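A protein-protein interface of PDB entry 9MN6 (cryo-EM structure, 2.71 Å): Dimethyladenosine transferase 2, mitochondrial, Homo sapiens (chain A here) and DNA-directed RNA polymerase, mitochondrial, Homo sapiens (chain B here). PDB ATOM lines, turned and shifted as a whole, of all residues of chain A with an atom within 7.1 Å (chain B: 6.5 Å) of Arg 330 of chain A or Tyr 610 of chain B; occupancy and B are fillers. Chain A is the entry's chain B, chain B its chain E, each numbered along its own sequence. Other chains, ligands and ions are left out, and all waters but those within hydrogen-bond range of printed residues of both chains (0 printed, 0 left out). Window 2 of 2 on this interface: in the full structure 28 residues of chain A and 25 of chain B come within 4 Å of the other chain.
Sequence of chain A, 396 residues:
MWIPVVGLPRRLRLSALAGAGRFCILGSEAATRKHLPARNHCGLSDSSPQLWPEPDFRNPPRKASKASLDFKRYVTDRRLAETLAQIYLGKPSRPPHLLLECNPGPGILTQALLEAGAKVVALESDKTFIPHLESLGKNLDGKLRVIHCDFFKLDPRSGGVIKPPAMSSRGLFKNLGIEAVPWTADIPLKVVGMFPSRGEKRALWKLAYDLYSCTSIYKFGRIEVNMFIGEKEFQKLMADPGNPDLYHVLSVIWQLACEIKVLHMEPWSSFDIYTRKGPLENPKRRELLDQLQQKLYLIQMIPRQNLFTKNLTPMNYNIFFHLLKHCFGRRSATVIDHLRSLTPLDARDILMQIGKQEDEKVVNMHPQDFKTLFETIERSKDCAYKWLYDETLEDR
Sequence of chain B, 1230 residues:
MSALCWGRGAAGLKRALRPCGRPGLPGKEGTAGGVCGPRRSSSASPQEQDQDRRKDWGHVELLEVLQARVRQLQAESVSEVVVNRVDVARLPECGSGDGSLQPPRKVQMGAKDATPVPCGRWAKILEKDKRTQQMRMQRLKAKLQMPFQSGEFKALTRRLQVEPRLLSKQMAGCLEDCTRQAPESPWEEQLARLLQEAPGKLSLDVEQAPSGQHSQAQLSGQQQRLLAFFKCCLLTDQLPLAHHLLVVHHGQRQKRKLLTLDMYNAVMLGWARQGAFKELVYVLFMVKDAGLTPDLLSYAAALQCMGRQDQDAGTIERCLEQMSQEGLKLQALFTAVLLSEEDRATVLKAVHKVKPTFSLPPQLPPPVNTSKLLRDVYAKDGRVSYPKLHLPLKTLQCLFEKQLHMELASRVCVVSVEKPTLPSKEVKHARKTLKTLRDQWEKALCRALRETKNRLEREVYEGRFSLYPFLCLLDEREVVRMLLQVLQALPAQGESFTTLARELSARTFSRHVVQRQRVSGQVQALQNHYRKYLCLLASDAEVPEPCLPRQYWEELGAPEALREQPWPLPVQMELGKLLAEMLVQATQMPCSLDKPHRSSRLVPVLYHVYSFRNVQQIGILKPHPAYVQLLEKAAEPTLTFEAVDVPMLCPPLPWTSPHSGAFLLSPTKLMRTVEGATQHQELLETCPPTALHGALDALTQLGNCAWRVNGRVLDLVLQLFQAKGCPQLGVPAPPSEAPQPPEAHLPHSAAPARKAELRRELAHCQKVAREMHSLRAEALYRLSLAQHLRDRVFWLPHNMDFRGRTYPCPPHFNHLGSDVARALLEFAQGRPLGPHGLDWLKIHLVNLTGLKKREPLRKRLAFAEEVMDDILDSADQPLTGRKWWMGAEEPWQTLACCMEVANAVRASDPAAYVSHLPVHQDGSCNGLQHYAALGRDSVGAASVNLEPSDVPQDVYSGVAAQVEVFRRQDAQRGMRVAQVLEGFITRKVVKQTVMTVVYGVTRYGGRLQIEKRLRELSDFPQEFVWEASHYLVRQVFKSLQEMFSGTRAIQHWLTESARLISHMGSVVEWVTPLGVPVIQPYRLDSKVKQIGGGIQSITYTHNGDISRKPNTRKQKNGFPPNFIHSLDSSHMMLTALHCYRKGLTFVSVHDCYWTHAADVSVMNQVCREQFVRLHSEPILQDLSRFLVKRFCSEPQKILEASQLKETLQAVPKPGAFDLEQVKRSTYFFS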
ATOM      1  N   HIS A 322      10.000   7.723  -1.259  1.00  0.00           N
ATOM      2  CA  HIS A 322      10.591   8.964  -0.775  1.00  0.00           C
ATOM      3  C   HIS A 322       9.566  10.087  -0.711  1.00  0.00           C
ATOM      4  O   HIS A 322       9.638  10.931   0.188  1.00  0.00           O
ATOM      5  CB  HIS A 322      11.760   9.383  -1.658  1.00  0.00           C
ATOM      6  CG  HIS A 322      12.623  10.433  -1.036  1.00  0.00           C
ATOM      7  ND1 HIS A 322      13.338  10.215   0.120  1.00  0.00           N
ATOM      8  CD2 HIS A 322      12.868  11.716  -1.395  1.00  0.00           C
ATOM      9  CE1 HIS A 322      14.002  11.311   0.437  1.00  0.00           C
ATOM     10  NE2 HIS A 322      13.733  12.238  -0.464  1.00  0.00           N
ATOM     11  N   LYS A 325       7.704   9.398   2.586  1.00  0.00           N
ATOM     12  CA  LYS A 325       8.401   9.664   3.840  1.00  0.00           C
ATOM     13  C   LYS A 325       8.753  11.144   3.968  1.00  0.00           C
ATOM     14  O   LYS A 325       8.749  11.692   5.077  1.00  0.00           O
ATOM     15  CB  LYS A 325       9.643   8.786   3.970  1.00  0.00           C
ATOM     16  CG  LYS A 325      10.373   9.022   5.274  1.00  0.00           C
ATOM     17  CD  LYS A 325       9.472   8.522   6.403  1.00  0.00           C
ATOM     18  CE  LYS A 325      10.130   8.565   7.766  1.00  0.00           C
ATOM     19  NZ  LYS A 325      10.392   9.948   8.215  1.00  0.00           N
ATOM     20  N   HIS A 326       9.009  11.825   2.847  1.00  0.00           N
ATOM     21  CA  HIS A 326       9.213  13.265   2.902  1.00  0.00           C
ATOM     22  C   HIS A 326       7.931  13.992   3.284  1.00  0.00           C
ATOM     23  O   HIS A 326       7.973  14.957   4.054  1.00  0.00           O
ATOM     24  CB  HIS A 326       9.731  13.785   1.564  1.00  0.00           C
ATOM     25  CG  HIS A 326      10.259  15.184   1.635  1.00  0.00           C
ATOM     26  ND1 HIS A 326       9.766  16.206   0.855  1.00  0.00           N
ATOM     27  CD2 HIS A 326      11.229  15.732   2.403  1.00  0.00           C
ATOM     28  CE1 HIS A 326      10.410  17.322   1.136  1.00  0.00           C
ATOM     29  NE2 HIS A 326      11.305  17.063   2.071  1.00  0.00           N
ATOM     30  N   CYS A 327       6.785  13.547   2.755  1.00  0.00           N
ATOM     31  CA  CYS A 327       5.512  14.176   3.092  1.00  0.00           C
ATOM     32  C   CYS A 327       5.161  13.962   4.558  1.00  0.00           C
ATOM     33  O   CYS A 327       4.600  14.853   5.207  1.00  0.00           O
ATOM     34  CB  CYS A 327       4.403  13.631   2.194  1.00  0.00           C
ATOM     35  SG  CYS A 327       4.234  14.479   0.606  1.00  0.00           S
ATOM     36  N   PHE A 328       5.485  12.793   5.096  1.00  0.00           N
ATOM     37  CA  PHE A 328       5.215  12.500   6.494  1.00  0.00           C
ATOM     38  C   PHE A 328       6.365  12.850   7.431  1.00  0.00           C
ATOM     39  O   PHE A 328       6.270  12.566   8.629  1.00  0.00           O
ATOM     40  CB  PHE A 328       4.859  11.026   6.653  1.00  0.00           C
ATOM     41  CG  PHE A 328       3.453  10.686   6.245  1.00  0.00           C
ATOM     42  CD1 PHE A 328       2.392  10.977   7.085  1.00  0.00           C
ATOM     43  CD2 PHE A 328       3.190  10.067   5.036  1.00  0.00           C
ATOM     44  CE1 PHE A 328       1.096  10.662   6.727  1.00  0.00           C
ATOM     45  CE2 PHE A 328       1.893   9.753   4.672  1.00  0.00           C
ATOM     46  CZ  PHE A 328       0.847  10.051   5.520  1.00  0.00           C
ATOM     47  N   GLY A 329       7.450  13.436   6.923  1.00  0.00           N
ATOM     48  CA  GLY A 329       8.485  13.944   7.810  1.00  0.00           C
ATOM     49  C   GLY A 329       8.003  15.121   8.635  1.00  0.00           C
ATOM     50  O   GLY A 329       8.281  15.209   9.834  1.00  0.00           O
ATOM     51  N   ARG A 330       7.276  16.038   8.006  1.00  0.00           N
ATOM     52  CA  ARG A 330       6.579  17.124   8.688  1.00  0.00           C
ATOM     53  C   ARG A 330       5.090  16.833   8.552  1.00  0.00           C
ATOM     54  O   ARG A 330       4.500  17.072   7.494  1.00  0.00           O
ATOM     55  CB  ARG A 330       6.942  18.478   8.088  1.00  0.00           C
ATOM     56  CG  ARG A 330       7.903  19.296   8.921  1.00  0.00           C
ATOM     57  CD  ARG A 330       8.265  20.587   8.213  1.00  0.00           C
ATOM     58  NE  ARG A 330       8.928  20.327   6.942  1.00  0.00           N
ATOM     59  CZ  ARG A 330       8.591  20.888   5.790  1.00  0.00           C
ATOM     60  NH1 ARG A 330       7.605  21.767   5.713  1.00  0.00           N
ATOM     61  NH2 ARG A 330       9.260  20.561   4.689  1.00  0.00           N
ATOM     62  N   ARG A 331       4.487  16.310   9.621  1.00  0.00           N
ATOM     63  CA  ARG A 331       3.093  15.887   9.545  1.00  0.00           C
ATOM     64  C   ARG A 331       2.144  17.076   9.520  1.00  0.00           C
ATOM     65  O   ARG A 331       1.098  17.019   8.863  1.00  0.00           O
ATOM     66  CB  ARG A 331       2.769  14.969  10.720  1.00  0.00           C
ATOM     67  CG  ARG A 331       3.804  13.876  10.929  1.00  0.00           C
ATOM     68  CD  ARG A 331       3.507  13.001  12.158  1.00  0.00           C
ATOM     69  NE  ARG A 331       2.135  12.510  12.320  1.00  0.00           N
ATOM     70  CZ  ARG A 331       1.396  11.871  11.414  1.00  0.00           C
ATOM     71  NH1 ARG A 331       1.903  11.437  10.272  1.00  0.00           N
ATOM     72  NH2 ARG A 331       0.122  11.609  11.690  1.00  0.00           N
ATOM     73  N   SER A 332       2.488  18.158  10.221  1.00  0.00           N
ATOM     74  CA  SER A 332       1.637  19.339  10.261  1.00  0.00           C
ATOM     75  C   SER A 332       1.692  20.158   8.978  1.00  0.00           C
ATOM     76  O   SER A 332       0.808  20.993   8.759  1.00  0.00           O
ATOM     77  CB  SER A 332       2.023  20.223  11.448  1.00  0.00           C
ATOM     78  OG  SER A 332       3.061  21.121  11.096  1.00  0.00           O
ATOM     79  N   ALA A 333       2.699  19.948   8.136  1.00  0.00           N
ATOM     80  CA  ALA A 333       2.825  20.732   6.919  1.00  0.00           C
ATOM     81  C   ALA A 333       1.812  20.275   5.874  1.00  0.00           C
ATOM     82  O   ALA A 333       1.189  19.218   5.991  1.00  0.00           O
ATOM     83  CB  ALA A 333       4.241  20.634   6.357  1.00  0.00           C
ATOM     84  N   THR A 334       1.642  21.101   4.850  1.00  0.00           N
ATOM     85  CA  THR A 334       0.720  20.804   3.767  1.00  0.00           C
ATOM     86  C   THR A 334       1.453  20.164   2.592  1.00  0.00           C
ATOM     87  O   THR A 334       2.676  20.015   2.587  1.00  0.00           O
ATOM     88  CB  THR A 334      -0.010  22.070   3.320  1.00  0.00           C
ATOM     89  OG1 THR A 334      -1.022  21.727   2.365  1.00  0.00           O
ATOM     90  CG2 THR A 334       0.959  23.065   2.702  1.00  0.00           C
ATOM     91  N   ASP A 337       3.975  22.501   0.837  1.00  0.00           N
ATOM     92  CA  ASP A 337       5.272  22.647   1.493  1.00  0.00           C
ATOM     93  C   ASP A 337       6.228  21.522   1.117  1.00  0.00           C
ATOM     94  O   ASP A 337       7.420  21.758   0.894  1.00  0.00           O
ATOM     95  CB  ASP A 337       5.088  22.687   3.011  1.00  0.00           C
ATOM     96  CG  ASP A 337       4.364  23.932   3.482  1.00  0.00           C
ATOM     97  OD1 ASP A 337       3.872  24.698   2.627  1.00  0.00           O
ATOM     98  OD2 ASP A 337       4.281  24.137   4.711  1.00  0.00           O
ATOM     99  N   HIS A 338       5.726  20.291   1.058  1.00  0.00           N
ATOM    100  CA  HIS A 338       6.584  19.161   0.732  1.00  0.00           C
ATOM    101  C   HIS A 338       6.879  19.082  -0.758  1.00  0.00           C
ATOM    102  O   HIS A 338       7.986  18.691  -1.147  1.00  0.00           O
ATOM    103  CB  HIS A 338       5.940  17.871   1.230  1.00  0.00           C
ATOM    104  CG  HIS A 338       5.864  17.786   2.720  1.00  0.00           C
ATOM    105  ND1 HIS A 338       6.962  17.524   3.508  1.00  0.00           N
ATOM    106  CD2 HIS A 338       4.823  17.953   3.568  1.00  0.00           C
ATOM    107  CE1 HIS A 338       6.600  17.527   4.778  1.00  0.00           C
ATOM    108  NE2 HIS A 338       5.306  17.779   4.841  1.00  0.00           N
ATOM    109  N   SER A 341       9.627  21.259  -2.119  1.00  0.00           N
ATOM    110  CA  SER A 341      10.936  20.653  -1.926  1.00  0.00           C
ATOM    111  C   SER A 341      11.120  19.380  -2.741  1.00  0.00           C
ATOM    112  O   SER A 341      12.261  18.946  -2.930  1.00  0.00           O
ATOM    113  CB  SER A 341      11.158  20.353  -0.445  1.00  0.00           C
ATOM    114  OG  SER A 341      11.112  21.539   0.329  1.00  0.00           O
ATOM    115  N   LEU A 342      10.035  18.776  -3.228  1.00  0.00           N
ATOM    116  CA  LEU A 342      10.134  17.506  -3.938  1.00  0.00           C
ATOM    117  C   LEU A 342      10.243  17.648  -5.450  1.00  0.00           C
ATOM    118  O   LEU A 342      10.895  16.812  -6.085  1.00  0.00           O
ATOM    119  CB  LEU A 342       8.926  16.623  -3.617  1.00  0.00           C
ATOM    120  CG  LEU A 342       9.040  15.726  -2.386  1.00  0.00           C
ATOM    121  CD1 LEU A 342       7.891  14.736  -2.344  1.00  0.00           C
ATOM    122  CD2 LEU A 342      10.381  15.008  -2.343  1.00  0.00           C
ATOM    123  N   LYS A 361      -3.736  19.068   4.114  1.00  0.00           N
ATOM    124  CA  LYS A 361      -2.686  18.620   5.013  1.00  0.00           C
ATOM    125  C   LYS A 361      -2.329  17.173   4.677  1.00  0.00           C
ATOM    126  O   LYS A 361      -3.117  16.448   4.065  1.00  0.00           O
ATOM    127  CB  LYS A 361      -3.148  18.762   6.471  1.00  0.00           C
ATOM    128  CG  LYS A 361      -2.071  18.624   7.545  1.00  0.00           C
ATOM    129  CD  LYS A 361      -2.658  18.725   8.946  1.00  0.00           C
ATOM    130  CE  LYS A 361      -3.524  19.963   9.100  1.00  0.00           C
ATOM    131  NZ  LYS A 361      -4.069  20.093  10.477  1.00  0.00           N
ATOM    132  N   VAL A 362      -1.112  16.773   5.057  1.00  0.00           N
ATOM    133  CA  VAL A 362      -0.609  15.441   4.726  1.00  0.00           C
ATOM    134  C   VAL A 362      -1.430  14.357   5.419  1.00  0.00           C
ATOM    135  O   VAL A 362      -1.784  13.341   4.806  1.00  0.00           O
ATOM    136  CB  VAL A 362       0.885  15.338   5.080  1.00  0.00           C
ATOM    137  CG1 VAL A 362       1.417  13.946   4.777  1.00  0.00           C
ATOM    138  CG2 VAL A 362       1.675  16.383   4.321  1.00  0.00           C
ATOM    139  N   VAL A 363      -1.774  14.562   6.695  1.00  0.00           N
ATOM    140  CA  VAL A 363      -2.460  13.523   7.464  1.00  0.00           C
ATOM    141  C   VAL A 363      -3.930  13.381   7.114  1.00  0.00           C
ATOM    142  O   VAL A 363      -4.591  12.473   7.635  1.00  0.00           O
ATOM    143  CB  VAL A 363      -2.356  13.776   8.981  1.00  0.00           C
ATOM    144  CG1 VAL A 363      -0.906  13.823   9.404  1.00  0.00           C
ATOM    145  CG2 VAL A 363      -3.082  15.056   9.362  1.00  0.00           C
ATOM    146  N   TYR A 389      14.659  13.207  -6.474  1.00  0.00           N
ATOM    147  CA  TYR A 389      15.157  12.048  -5.753  1.00  0.00           C
ATOM    148  C   TYR A 389      16.103  11.242  -6.633  1.00  0.00           C
ATOM    149  O   TYR A 389      15.873  11.062  -7.832  1.00  0.00           O
ATOM    150  CB  TYR A 389      14.009  11.168  -5.255  1.00  0.00           C
ATOM    151  CG  TYR A 389      14.467   9.851  -4.656  1.00  0.00           C
ATOM    152  CD1 TYR A 389      14.927   9.794  -3.349  1.00  0.00           C
ATOM    153  CD2 TYR A 389      14.405   8.663  -5.377  1.00  0.00           C
ATOM    154  CE1 TYR A 389      15.336   8.604  -2.782  1.00  0.00           C
ATOM    155  CE2 TYR A 389      14.816   7.465  -4.817  1.00  0.00           C
ATOM    156  CZ  TYR A 389      15.279   7.445  -3.517  1.00  0.00           C
ATOM    157  OH  TYR A 389      15.688   6.263  -2.948  1.00  0.00           O
ATOM    158  N   LEU A 393      20.614  10.447  -2.412  1.00  0.00           N
ATOM    159  CA  LEU A 393      19.929  10.841  -1.189  1.00  0.00           C
ATOM    160  C   LEU A 393      19.915   9.740  -0.137  1.00  0.00           C
ATOM    161  O   LEU A 393      19.305   9.936   0.920  1.00  0.00           O
ATOM    162  CB  LEU A 393      18.497  11.278  -1.496  1.00  0.00           C
ATOM    163  CG  LEU A 393      18.390  12.581  -2.288  1.00  0.00           C
ATOM    164  CD1 LEU A 393      16.941  12.904  -2.606  1.00  0.00           C
ATOM    165  CD2 LEU A 393      19.066  13.723  -1.553  1.00  0.00           C
ATOM    166  N   HIS B 608      15.650  21.889  -0.325  1.00  0.00           N
ATOM    167  CA  HIS B 608      15.857  21.308   0.996  1.00  0.00           C
ATOM    168  C   HIS B 608      15.106  19.987   1.058  1.00  0.00           C
ATOM    169  O   HIS B 608      13.906  19.946   1.330  1.00  0.00           O
ATOM    170  CB  HIS B 608      15.394  22.264   2.082  1.00  0.00           C
ATOM    171  CG  HIS B 608      15.755  21.821   3.460  1.00  0.00           C
ATOM    172  ND1 HIS B 608      14.872  21.154   4.280  1.00  0.00           N
ATOM    173  CD2 HIS B 608      16.903  21.947   4.165  1.00  0.00           C
ATOM    174  CE1 HIS B 608      15.460  20.891   5.432  1.00  0.00           C
ATOM    175  NE2 HIS B 608      16.694  21.359   5.388  1.00  0.00           N
ATOM    176  N   VAL B 609      15.819  18.896   0.811  1.00  0.00           N
ATOM    177  CA  VAL B 609      15.230  17.565   0.810  1.00  0.00           C
ATOM    178  C   VAL B 609      15.672  16.830   2.070  1.00  0.00           C
ATOM    179  O   VAL B 609      16.831  16.921   2.490  1.00  0.00           O
ATOM    180  CB  VAL B 609      15.587  16.792  -0.471  1.00  0.00           C
ATOM    181  CG1 VAL B 609      14.967  17.476  -1.674  1.00  0.00           C
ATOM    182  CG2 VAL B 609      17.091  16.725  -0.673  1.00  0.00           C
ATOM    183  N   TYR B 610      14.731  16.153   2.712  1.00  0.00           N
ATOM    184  CA  TYR B 610      15.078  15.286   3.825  1.00  0.00           C
ATOM    185  C   TYR B 610      15.687  14.000   3.286  1.00  0.00           C
ATOM    186  O   TYR B 610      15.085  13.325   2.448  1.00  0.00           O
ATOM    187  CB  TYR B 610      13.837  14.971   4.657  1.00  0.00           C
ATOM    188  CG  TYR B 610      13.279  16.129   5.455  1.00  0.00           C
ATOM    189  CD1 TYR B 610      14.044  17.258   5.720  1.00  0.00           C
ATOM    190  CD2 TYR B 610      11.973  16.096   5.929  1.00  0.00           C
ATOM    191  CE1 TYR B 610      13.526  18.312   6.450  1.00  0.00           C
ATOM    192  CE2 TYR B 610      11.448  17.146   6.661  1.00  0.00           C
ATOM    193  CZ  TYR B 610      12.229  18.251   6.914  1.00  0.00           C
ATOM    194  OH  TYR B 610      11.712  19.301   7.638  1.00  0.00           O
ATOM    195  N   SER B 611      16.879  13.655   3.761  1.00  0.00           N
ATOM    196  CA  SER B 611      17.517  12.388   3.446  1.00  0.00           C
ATOM    197  C   SER B 611      17.497  11.524   4.695  1.00  0.00           C
ATOM    198  O   SER B 611      17.635  12.025   5.816  1.00  0.00           O
ATOM    199  CB  SER B 611      18.950  12.572   2.950  1.00  0.00           C
ATOM    200  OG  SER B 611      18.973  13.284   1.727  1.00  0.00           O
ATOM    201  N   PHE B 612      17.309  10.227   4.499  1.00  0.00           N
ATOM    202  CA  PHE B 612      16.870   9.350   5.570  1.00  0.00           C
ATOM    203  C   PHE B 612      17.853   8.199   5.689  1.00  0.00           C
ATOM    204  O   PHE B 612      18.113   7.498   4.707  1.00  0.00           O
ATOM    205  CB  PHE B 612      15.466   8.839   5.271  1.00  0.00           C
ATOM    206  CG  PHE B 612      14.401   9.872   5.457  1.00  0.00           C
ATOM    207  CD1 PHE B 612      13.936  10.204   6.720  1.00  0.00           C
ATOM    208  CD2 PHE B 612      13.892  10.546   4.354  1.00  0.00           C
ATOM    209  CE1 PHE B 612      12.970  11.171   6.876  1.00  0.00           C
ATOM    210  CE2 PHE B 612      12.919  11.507   4.502  1.00  0.00           C
ATOM    211  CZ  PHE B 612      12.460  11.828   5.770  1.00  0.00           C
ATOM    212  N   GLN B 617      17.009  11.458  10.311  1.00  0.00           N
ATOM    213  CA  GLN B 617      16.497  12.327   9.253  1.00  0.00           C
ATOM    214  C   GLN B 617      17.365  13.577   9.201  1.00  0.00           C
ATOM    215  O   GLN B 617      17.358  14.372  10.146  1.00  0.00           O
ATOM    216  CB  GLN B 617      15.042  12.700   9.535  1.00  0.00           C
ATOM    217  CG  GLN B 617      14.470  13.806   8.667  1.00  0.00           C
ATOM    218  CD  GLN B 617      13.120  14.272   9.176  1.00  0.00           C
ATOM    219  OE1 GLN B 617      13.016  14.817  10.275  1.00  0.00           O
ATOM    220  NE2 GLN B 617      12.074  14.028   8.397  1.00  0.00           N
ATOM    221  N   ILE B 618      18.104  13.770   8.109  1.00  0.00           N
ATOM    222  CA  ILE B 618      19.012  14.905   7.980  1.00  0.00           C
ATOM    223  C   ILE B 618      18.585  15.757   6.789  1.00  0.00           C
ATOM    224  O   ILE B 618      18.172  15.230   5.752  1.00  0.00           O
ATOM    225  CB  ILE B 618      20.484  14.454   7.869  1.00  0.00           C
ATOM    226  CG1 ILE B 618      20.735  13.594   6.627  1.00  0.00           C
ATOM    227  CG2 ILE B 618      20.908  13.698   9.118  1.00  0.00           C
ATOM    228  CD1 ILE B 618      22.200  13.329   6.362  1.00  0.00           C
ATOM    229  N   GLY B 619      18.639  17.075   6.957  1.00  0.00           N
ATOM    230  CA  GLY B 619      18.296  17.972   5.865  1.00  0.00           C
ATOM    231  C   GLY B 619      19.484  18.192   4.943  1.00  0.00           C
ATOM    232  O   GLY B 619      20.586  18.523   5.378  1.00  0.00           O
ATOM    233  N   ILE B 620      19.246  18.003   3.648  1.00  0.00           N
ATOM    234  CA  ILE B 620      20.279  18.080   2.625  1.00  0.00           C
ATOM    235  C   ILE B 620      19.857  19.125   1.605  1.00  0.00           C
ATOM    236  O   ILE B 620      18.728  19.090   1.102  1.00  0.00           O
ATOM    237  CB  ILE B 620      20.507  16.716   1.947  1.00  0.00           C
ATOM    238  CG1 ILE B 620      20.893  15.662   2.984  1.00  0.00           C
ATOM    239  CG2 ILE B 620      21.572  16.816   0.866  1.00  0.00           C
ATOM    240  CD1 ILE B 620      22.140  15.984   3.748  1.00  0.00           C
ATOM    241  N   ILE B1095      13.572  27.232   7.744  1.00  0.00           N
ATOM    242  CA  ILE B1095      13.532  25.973   7.007  1.00  0.00           C
ATOM    243  C   ILE B1095      13.376  24.793   7.958  1.00  0.00           C
ATOM    244  O   ILE B1095      12.393  24.049   7.872  1.00  0.00           O
ATOM    245  CB  ILE B1095      14.776  25.805   6.119  1.00  0.00           C
ATOM    246  CG1 ILE B1095      14.824  26.903   5.055  1.00  0.00           C
ATOM    247  CG2 ILE B1095      14.753  24.458   5.454  1.00  0.00           C
ATOM    248  CD1 ILE B1095      16.135  26.970   4.303  1.00  0.00           C
ATOM    249  N   GLN B1096      14.329  24.606   8.867  1.00  0.00           N
ATOM    250  CA  GLN B1096      14.236  23.507   9.821  1.00  0.00           C
ATOM    251  C   GLN B1096      14.922  23.913  11.118  1.00  0.00           C
ATOM    252  O   GLN B1096      15.371  25.050  11.284  1.00  0.00           O
ATOM    253  CB  GLN B1096      14.863  22.219   9.282  1.00  0.00           C
ATOM    254  CG  GLN B1096      16.362  22.298   9.057  1.00  0.00           C
ATOM    255  CD  GLN B1096      16.930  21.016   8.493  1.00  0.00           C
ATOM    256  OE1 GLN B1096      16.215  20.032   8.317  1.00  0.00           O
ATOM    257  NE2 GLN B1096      18.225  21.017   8.209  1.00  0.00           N
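The backbone carbonyl oxygen (O) of His 608 of chain B lies close to the side-chain hydroxyl (OG) of Ser 341 of chain A, at 3.4 Å. The backbone carbonyl oxygen (O) of Tyr 610 of chain B lies close to a ring nitrogen (NE2) of His 322 of chain A. OH of Tyr 610 of chain B sits at hydrogen-bond distance from NE of Arg 330 of chain A (3.0 Å). The backbone carbonyl oxygen (O) of Leu 393 of chain A lies close to the side-chain hydroxyl (OG) of Ser 611 of chain B (3.5 Å).
A ring nitrogen (NE2) of His 608 of chain B lies close to the side-chain amide nitrogen (NE2) of Gln 1096 of chain B, 3.2 Å away. The backbone carbonyl oxygen of Val 609 of chain B is in hydrogen-bond range of the backbone NH of Ile 620 of chain B (2.9 Å). The backbone NH (N) of Ser 611 of chain B sits at hydrogen-bond distance from the backbone carbonyl oxygen (O) of Ile 618 of chain B (2.8 Å). A ring nitrogen (ND1) of His 338 of chain A is in hydrogen-bond range of the backbone carbonyl oxygen of His 326 of chain A, 2.8 Å away. The backbone carbonyl oxygen (O) of Arg 330 of chain A is in hydrogen-bond range of a ring nitrogen (NE2) of His 338 of chain A, 2.9 Å away.
Among the printed residues, merely in contact across the chains: Lys 325 of chain A with Phe 612 of chain B (3.2 Å), Ser 341 of chain A with Val 609 of chain B (3.3 Å), His 326 of chain A with Tyr 610 of chain B (3.5 Å), Gly 329 of chain A with Gln 617 of chain B (3.6 Å), Leu 393 of chain A with Val 609 of chain B (3.7 Å), His 326 of chain A with His 608 of chain B (3.95 Å) and His 322 of chain A with Phe 612 of chain B (3.99 Å).
Of chain B, only Tyr 610 (3.0 Å) comes within 4 Å of Arg 330 of chain A. Of the printed residues of chain A, His 608 of chain B touches His 326 and Ser 341. Of chain A, only His 322, His 326 and Arg 330 come within 4 Å of Tyr 610 of chain B. Of the printed residues of chain A, Ser 611 of chain B touches Leu 393. Ile 618 of chain B touches none of the printed residues of chain A. Gln 1096 of chain B touches none of the printed residues of chain A. The nearest residue of chain B that does not touch Arg 330 of chain A is Ile 1095 of chain B (5.2 Å).
Hydrophobic or aromatic side chains of chain A that line the printed part of chain B: His 322, His 326 and Leu 393. Of the 11 printed residues of chain B, 6 touch a printed residue of chain A. Among the printed residues, no Asp or Glu carboxylate lies within 4 Å of a Lys or Arg side-chain nitrogen of the other chain.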
